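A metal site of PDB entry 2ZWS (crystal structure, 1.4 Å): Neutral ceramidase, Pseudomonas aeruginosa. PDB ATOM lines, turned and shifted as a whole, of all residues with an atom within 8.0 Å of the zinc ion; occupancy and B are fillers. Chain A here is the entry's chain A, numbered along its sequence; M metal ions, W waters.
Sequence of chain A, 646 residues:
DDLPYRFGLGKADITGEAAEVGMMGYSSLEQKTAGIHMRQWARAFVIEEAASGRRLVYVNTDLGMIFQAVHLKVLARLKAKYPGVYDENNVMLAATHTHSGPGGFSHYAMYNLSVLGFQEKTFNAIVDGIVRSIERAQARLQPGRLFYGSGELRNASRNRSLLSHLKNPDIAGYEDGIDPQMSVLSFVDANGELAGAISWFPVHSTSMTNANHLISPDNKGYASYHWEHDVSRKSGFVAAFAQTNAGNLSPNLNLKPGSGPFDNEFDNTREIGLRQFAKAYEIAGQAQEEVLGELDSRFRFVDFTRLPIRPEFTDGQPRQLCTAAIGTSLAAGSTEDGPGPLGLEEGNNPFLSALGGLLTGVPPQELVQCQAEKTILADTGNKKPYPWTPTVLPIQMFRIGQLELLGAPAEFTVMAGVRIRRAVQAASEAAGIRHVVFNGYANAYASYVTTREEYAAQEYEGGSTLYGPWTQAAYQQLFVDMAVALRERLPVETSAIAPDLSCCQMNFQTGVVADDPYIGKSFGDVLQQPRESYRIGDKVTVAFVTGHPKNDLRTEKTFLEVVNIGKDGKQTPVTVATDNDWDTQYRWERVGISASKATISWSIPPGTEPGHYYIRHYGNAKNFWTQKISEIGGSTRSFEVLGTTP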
ATOM      1  N   GLY A  25      -6.109  26.587 -19.072  1.00  0.00           N
ATOM      2  CA  GLY A  25      -5.898  25.206 -19.493  1.00  0.00           C
ATOM      3  C   GLY A  25      -6.577  24.885 -20.815  1.00  0.00           C
ATOM      4  O   GLY A  25      -5.981  24.214 -21.681  1.00  0.00           O
ATOM      5  N   GLY A  64      -3.082  25.161 -12.926  1.00  0.00           N
ATOM      6  CA  GLY A  64      -2.782  24.577 -14.235  1.00  0.00           C
ATOM      7  C   GLY A  64      -1.287  24.410 -14.417  1.00  0.00           C
ATOM      8  O   GLY A  64      -0.824  23.434 -15.015  1.00  0.00           O
ATOM      9  N   MET A  65      -0.526  25.359 -13.867  1.00  0.00           N
ATOM     10  CA  MET A  65       0.925  25.283 -13.978  1.00  0.00           C
ATOM     11  C   MET A  65       1.543  26.282 -13.032  1.00  0.00           C
ATOM     12  O   MET A  65       0.825  27.111 -12.433  1.00  0.00           O
ATOM     13  CB  MET A  65       1.382  25.511 -15.412  1.00  0.00           C
ATOM     14  CG  MET A  65       0.746  26.657 -16.087  1.00  0.00           C
ATOM     15  SD  MET A  65      -0.941  26.425 -16.803  1.00  0.00           S
ATOM     16  CE  MET A  65      -0.704  25.251 -18.127  1.00  0.00           C
ATOM     17  N   HIS A  97      -1.889  20.632 -12.481  1.00  0.00           N
ATOM     18  CA  HIS A  97      -2.384  20.771 -13.874  1.00  0.00           C
ATOM     19  C   HIS A  97      -3.907  20.684 -13.949  1.00  0.00           C
ATOM     20  O   HIS A  97      -4.471  20.260 -14.959  1.00  0.00           O
ATOM     21  CB  HIS A  97      -1.708  19.765 -14.788  1.00  0.00           C
ATOM     22  CG  HIS A  97      -1.771  20.120 -16.238  1.00  0.00           C
ATOM     23  ND1 HIS A  97      -1.605  21.403 -16.709  1.00  0.00           N
ATOM     24  CD2 HIS A  97      -1.836  19.318 -17.339  1.00  0.00           C
ATOM     25  CE1 HIS A  97      -1.644  21.383 -18.043  1.00  0.00           C
ATOM     26  NE2 HIS A  97      -1.772  20.128 -18.439  1.00  0.00           N
ATOM     27  N   HIS A  99      -7.415  22.129 -14.848  1.00  0.00           N
ATOM     28  CA  HIS A  99      -7.803  23.067 -15.893  1.00  0.00           C
ATOM     29  C   HIS A  99      -9.008  23.914 -15.471  1.00  0.00           C
ATOM     30  O   HIS A  99      -9.629  24.539 -16.318  1.00  0.00           O
ATOM     31  CB  HIS A  99      -8.104  22.289 -17.179  1.00  0.00           C
ATOM     32  CG  HIS A  99      -6.887  21.741 -17.840  1.00  0.00           C
ATOM     33  ND1 HIS A  99      -5.932  21.008 -17.171  1.00  0.00           N
ATOM     34  CD2 HIS A  99      -6.478  21.804 -19.129  1.00  0.00           C
ATOM     35  CE1 HIS A  99      -4.977  20.637 -18.022  1.00  0.00           C
ATOM     36  NE2 HIS A  99      -5.272  21.140 -19.207  1.00  0.00           N
ATOM     37  N   ARG A 160      -3.583   9.617 -24.810  1.00  0.00           N
ATOM     38  CA  ARG A 160      -4.443  10.357 -25.751  1.00  0.00           C
ATOM     39  C   ARG A 160      -3.787  10.572 -27.111  1.00  0.00           C
ATOM     40  O   ARG A 160      -4.381  11.147 -28.034  1.00  0.00           O
ATOM     41  CB  ARG A 160      -4.874  11.688 -25.106  1.00  0.00           C
ATOM     42  CG  ARG A 160      -3.753  12.655 -24.966  1.00  0.00           C
ATOM     43  CD  ARG A 160      -4.152  13.910 -24.234  1.00  0.00           C
ATOM     44  NE  ARG A 160      -3.085  14.900 -24.338  1.00  0.00           N
ATOM     45  CZ  ARG A 160      -3.144  16.118 -23.779  1.00  0.00           C
ATOM     46  NH1 ARG A 160      -4.206  16.496 -23.061  1.00  0.00           N
ATOM     47  NH2 ARG A 160      -2.130  16.954 -23.960  1.00  0.00           N
ATOM     48  N   HIS A 204      -3.649  13.791 -16.765  1.00  0.00           N
ATOM     49  CA  HIS A 204      -4.216  15.135 -16.876  1.00  0.00           C
ATOM     50  C   HIS A 204      -5.369  15.345 -15.891  1.00  0.00           C
ATOM     51  O   HIS A 204      -6.253  14.493 -15.749  1.00  0.00           O
ATOM     52  CB  HIS A 204      -4.693  15.471 -18.298  1.00  0.00           C
ATOM     53  CG  HIS A 204      -3.661  16.177 -19.109  1.00  0.00           C
ATOM     54  ND1 HIS A 204      -2.534  15.552 -19.603  1.00  0.00           N
ATOM     55  CD2 HIS A 204      -3.595  17.474 -19.521  1.00  0.00           C
ATOM     56  CE1 HIS A 204      -1.799  16.441 -20.253  1.00  0.00           C
ATOM     57  NE2 HIS A 204      -2.415  17.612 -20.207  1.00  0.00           N
ATOM     58  N   SER A 205      -5.344  16.503 -15.236  1.00  0.00           N
ATOM     59  CA  SER A 205      -6.401  16.869 -14.316  1.00  0.00           C
ATOM     60  C   SER A 205      -7.481  17.657 -15.062  1.00  0.00           C
ATOM     61  O   SER A 205      -7.704  18.879 -14.837  1.00  0.00           O
ATOM     62  CB  SER A 205      -5.805  17.669 -13.140  1.00  0.00           C
ATOM     63  OG  SER A 205      -5.017  16.782 -12.347  1.00  0.00           O
ATOM     64  N   THR A 206      -8.186  16.928 -15.913  1.00  0.00           N
ATOM     65  CA  THR A 206      -9.118  17.529 -16.892  1.00  0.00           C
ATOM     66  C   THR A 206     -10.469  16.837 -16.798  1.00  0.00           C
ATOM     67  O   THR A 206     -11.237  16.829 -17.758  1.00  0.00           O
ATOM     68  CB  THR A 206      -8.589  17.336 -18.325  1.00  0.00           C
ATOM     69  OG1 THR A 206      -8.231  15.952 -18.524  1.00  0.00           O
ATOM     70  CG2 THR A 206      -7.361  18.194 -18.596  1.00  0.00           C
ATOM     71  N   GLN A 243       2.100  15.485 -10.246  1.00  0.00           N
ATOM     72  CA  GLN A 243       2.280  14.899 -11.586  1.00  0.00           C
ATOM     73  C   GLN A 243       3.665  14.305 -11.809  1.00  0.00           C
ATOM     74  O   GLN A 243       4.621  14.674 -11.113  1.00  0.00           O
ATOM     75  CB  GLN A 243       2.075  15.966 -12.682  1.00  0.00           C
ATOM     76  CG  GLN A 243       0.658  16.498 -12.724  1.00  0.00           C
ATOM     77  CD  GLN A 243      -0.321  15.551 -13.377  1.00  0.00           C
ATOM     78  OE1 GLN A 243       0.034  14.420 -13.790  1.00  0.00           O
ATOM     79  NE2 GLN A 243      -1.562  16.017 -13.511  1.00  0.00           N
ATOM     80  N   ALA A 246       3.009  13.492 -17.735  1.00  0.00           N
ATOM     81  CA  ALA A 246       1.585  13.340 -18.095  1.00  0.00           C
ATOM     82  C   ALA A 246       1.204  13.966 -19.442  1.00  0.00           C
ATOM     83  O   ALA A 246       0.014  14.068 -19.763  1.00  0.00           O
ATOM     84  CB  ALA A 246       0.717  13.938 -16.983  1.00  0.00           C
ATOM     85  N   GLY A 247       2.198  14.365 -20.225  1.00  0.00           N
ATOM     86  CA  GLY A 247       1.939  15.144 -21.435  1.00  0.00           C
ATOM     87  C   GLY A 247       0.940  14.484 -22.376  1.00  0.00           C
ATOM     88  O   GLY A 247       0.132  15.185 -23.031  1.00  0.00           O
ATOM     89  N   ASN A 248       0.991  13.159 -22.482  1.00  0.00           N
ATOM     90  CA  ASN A 248       0.100  12.470 -23.409  1.00  0.00           C
ATOM     91  C   ASN A 248      -0.891  11.549 -22.699  1.00  0.00           C
ATOM     92  O   ASN A 248      -1.400  10.594 -23.286  1.00  0.00           O
ATOM     93  CB  ASN A 248       0.892  11.697 -24.525  1.00  0.00           C
ATOM     94  CG  ASN A 248       1.981  10.760 -23.956  1.00  0.00           C
ATOM     95  OD1 ASN A 248       2.241  10.748 -22.747  1.00  0.00           O
ATOM     96  ND2 ASN A 248       2.595   9.955 -24.839  1.00  0.00           N
ATOM     97  N   LEU A 249      -1.204  11.868 -21.425  1.00  0.00           N
ATOM     98  CA  LEU A 249      -2.080  11.018 -20.610  1.00  0.00           C
ATOM     99  C   LEU A 249      -3.325  11.765 -20.118  1.00  0.00           C
ATOM    100  O   LEU A 249      -3.232  12.797 -19.441  1.00  0.00           O
ATOM    101  CB  LEU A 249      -1.317  10.474 -19.397  1.00  0.00           C
ATOM    102  CG  LEU A 249      -0.211   9.458 -19.664  1.00  0.00           C
ATOM    103  CD1 LEU A 249       0.603   9.259 -18.383  1.00  0.00           C
ATOM    104  CD2 LEU A 249      -0.828   8.139 -20.048  1.00  0.00           C
ATOM    105  N   ALA A 410       7.830  21.682 -17.779  1.00  0.00           N
ATOM    106  CA  ALA A 410       6.995  21.438 -18.959  1.00  0.00           C
ATOM    107  C   ALA A 410       6.141  20.164 -18.766  1.00  0.00           C
ATOM    108  O   ALA A 410       6.203  19.509 -17.720  1.00  0.00           O
ATOM    109  CB  ALA A 410       7.867  21.299 -20.234  1.00  0.00           C
ATOM    110  N   GLU A 411       5.335  19.842 -19.788  1.00  0.00           N
ATOM    111  CA  GLU A 411       4.549  18.600 -19.829  1.00  0.00           C
ATOM    112  C   GLU A 411       5.312  17.577 -20.630  1.00  0.00           C
ATOM    113  O   GLU A 411       5.396  17.708 -21.847  1.00  0.00           O
ATOM    114  CB  GLU A 411       3.184  18.816 -20.503  1.00  0.00           C
ATOM    115  CG  GLU A 411       2.483  20.106 -20.138  1.00  0.00           C
ATOM    116  CD  GLU A 411       0.982  20.018 -20.313  1.00  0.00           C
ATOM    117  OE1 GLU A 411       0.365  18.906 -20.204  1.00  0.00           O
ATOM    118  OE2 GLU A 411       0.390  21.083 -20.529  1.00  0.00           O
ATOM    119  N   TYR A 441       5.705  19.995 -14.737  1.00  0.00           N
ATOM    120  CA  TYR A 441       4.909  21.151 -14.279  1.00  0.00           C
ATOM    121  C   TYR A 441       5.556  21.857 -13.084  1.00  0.00           C
ATOM    122  O   TYR A 441       4.844  22.358 -12.213  1.00  0.00           O
ATOM    123  CB  TYR A 441       3.480  20.755 -13.903  1.00  0.00           C
ATOM    124  CG  TYR A 441       2.779  19.925 -14.956  1.00  0.00           C
ATOM    125  CD1 TYR A 441       2.079  20.530 -15.993  1.00  0.00           C
ATOM    126  CD2 TYR A 441       2.861  18.529 -14.925  1.00  0.00           C
ATOM    127  CE1 TYR A 441       1.432  19.751 -16.990  1.00  0.00           C
ATOM    128  CE2 TYR A 441       2.243  17.739 -15.900  1.00  0.00           C
ATOM    129  CZ  TYR A 441       1.544  18.353 -16.938  1.00  0.00           C
ATOM    130  OH  TYR A 441       0.963  17.544 -17.872  1.00  0.00           O
ATOM    131  N   TYR A 445       6.574  27.073 -16.930  1.00  0.00           N
ATOM    132  CA  TYR A 445       5.803  26.270 -17.876  1.00  0.00           C
ATOM    133  C   TYR A 445       6.210  26.615 -19.291  1.00  0.00           C
ATOM    134  O   TYR A 445       6.092  27.757 -19.710  1.00  0.00           O
ATOM    135  CB  TYR A 445       4.317  26.529 -17.672  1.00  0.00           C
ATOM    136  CG  TYR A 445       3.482  25.694 -18.595  1.00  0.00           C
ATOM    137  CD1 TYR A 445       3.213  24.344 -18.310  1.00  0.00           C
ATOM    138  CD2 TYR A 445       2.990  26.235 -19.775  1.00  0.00           C
ATOM    139  CE1 TYR A 445       2.463  23.553 -19.216  1.00  0.00           C
ATOM    140  CE2 TYR A 445       2.212  25.481 -20.645  1.00  0.00           C
ATOM    141  CZ  TYR A 445       1.965  24.147 -20.371  1.00  0.00           C
ATOM    142  OH  TYR A 445       1.218  23.400 -21.242  1.00  0.00           O
ATOM    143  N   SER A 447       5.218  24.574 -22.161  1.00  0.00           N
ATOM    144  CA  SER A 447       4.421  23.710 -23.041  1.00  0.00           C
ATOM    145  C   SER A 447       4.847  22.233 -22.979  1.00  0.00           C
ATOM    146  O   SER A 447       5.063  21.726 -21.925  1.00  0.00           O
ATOM    147  CB  SER A 447       4.390  24.308 -24.453  1.00  0.00           C
ATOM    148  OG  SER A 447       3.711  25.565 -24.417  1.00  0.00           O
ATOM    149  N   TYR A 448       4.985  21.559 -24.120  1.00  0.00           N
ATOM    150  CA  TYR A 448       5.102  20.094 -24.142  1.00  0.00           C
ATOM    151  C   TYR A 448       6.488  19.586 -24.525  1.00  0.00           C
ATOM    152  O   TYR A 448       7.256  20.279 -25.196  1.00  0.00           O
ATOM    153  CB  TYR A 448       4.014  19.457 -25.036  1.00  0.00           C
ATOM    154  CG  TYR A 448       2.624  19.522 -24.431  1.00  0.00           C
ATOM    155  CD1 TYR A 448       1.858  20.689 -24.477  1.00  0.00           C
ATOM    156  CD2 TYR A 448       2.058  18.400 -23.829  1.00  0.00           C
ATOM    157  CE1 TYR A 448       0.557  20.746 -23.871  1.00  0.00           C
ATOM    158  CE2 TYR A 448       0.785  18.419 -23.279  1.00  0.00           C
ATOM    159  CZ  TYR A 448       0.020  19.601 -23.276  1.00  0.00           C
ATOM    160  OH  TYR A 448      -1.247  19.595 -22.663  1.00  0.00           O
ATOM    161  N   TYR A 460      -0.780  16.532 -31.151  1.00  0.00           N
ATOM    162  CA  TYR A 460      -0.898  17.792 -30.416  1.00  0.00           C
ATOM    163  C   TYR A 460       0.365  18.132 -29.603  1.00  0.00           C
ATOM    164  O   TYR A 460       0.881  19.248 -29.674  1.00  0.00           O
ATOM    165  CB  TYR A 460      -2.143  17.738 -29.528  1.00  0.00           C
ATOM    166  CG  TYR A 460      -2.269  18.944 -28.627  1.00  0.00           C
ATOM    167  CD1 TYR A 460      -2.668  20.185 -29.129  1.00  0.00           C
ATOM    168  CD2 TYR A 460      -1.991  18.832 -27.269  1.00  0.00           C
ATOM    169  CE1 TYR A 460      -2.760  21.310 -28.291  1.00  0.00           C
ATOM    170  CE2 TYR A 460      -2.106  19.932 -26.408  1.00  0.00           C
ATOM    171  CZ  TYR A 460      -2.476  21.158 -26.939  1.00  0.00           C
ATOM    172  OH  TYR A 460      -2.580  22.255 -26.088  1.00  0.00           O
ATOM    173  N   GLU A 461       0.875  17.155 -28.865  1.00  0.00           N
ATOM    174  CA  GLU A 461       2.064  17.353 -28.029  1.00  0.00           C
ATOM    175  C   GLU A 461       3.316  17.707 -28.825  1.00  0.00           C
ATOM    176  O   GLU A 461       4.146  18.518 -28.382  1.00  0.00           O
ATOM    177  CB  GLU A 461       2.309  16.131 -27.149  1.00  0.00           C
ATOM    178  CG  GLU A 461       1.146  15.794 -26.203  1.00  0.00           C
ATOM    179  CD  GLU A 461      -0.006  15.043 -26.866  1.00  0.00           C
ATOM    180  OE1 GLU A 461       0.157  14.528 -28.011  1.00  0.00           O
ATOM    181  OE2 GLU A 461      -1.095  14.998 -26.278  1.00  0.00           O
HETATM  182 ZN    ZN M   1      -1.581  19.523 -20.520  1.00  0.00          ZN
HETATM  183  O   HOH W   1      -3.226  20.773 -20.983  1.00  0.00           O
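OE1 of Glu 411 lies close to OH of Tyr 441 (2.8 Å).
OE2 of Glu 411 sits close to OH of Tyr 445 (2.6 Å).
N of Glu 411 lies within hydrogen-bond range of O of Ser 447 (2.9 Å).
ND1 of His 204 lies within hydrogen-bond range of O of Ala 246 (3.0 Å).
ND1 of His 204 lies within hydrogen-bond range of O of Leu 249 (2.8 Å).
The side-chain hydroxyl of Tyr 448 sits close to the guanidinium group of Arg 160, 3.1 Å away.
The backbone carbonyl oxygen (O) of His 97 sits at hydrogen-bond distance from a ring nitrogen (ND1) of His 99, at 2.8 Å.
The backbone carbonyl oxygen (O) of Gly 64 sits at hydrogen-bond distance from a ring nitrogen (ND1) of His 97, 2.8 Å away.
Of the 22 residues printed, 4 come within 4 Å of the zinc ion.
The nearest printed residue that does not touch the zinc ion is Tyr 441 (4.2 Å).
The zinc ion is bound by OE1 of Glu 411, 2.1 Å away.
NE2 of His 204 is bound to the zinc ion (2.1 Å).
The zinc ion is bound by water W1 (2.1 Å).
OH of Tyr 448 binds the zinc ion, 2.2 Å away.
A ring nitrogen (NE2) of His 97 binds the zinc ion (2.2 Å).
The zinc ion is bound by the side-chain carboxylate (OE2) of Glu 411, at 2.5 Å.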
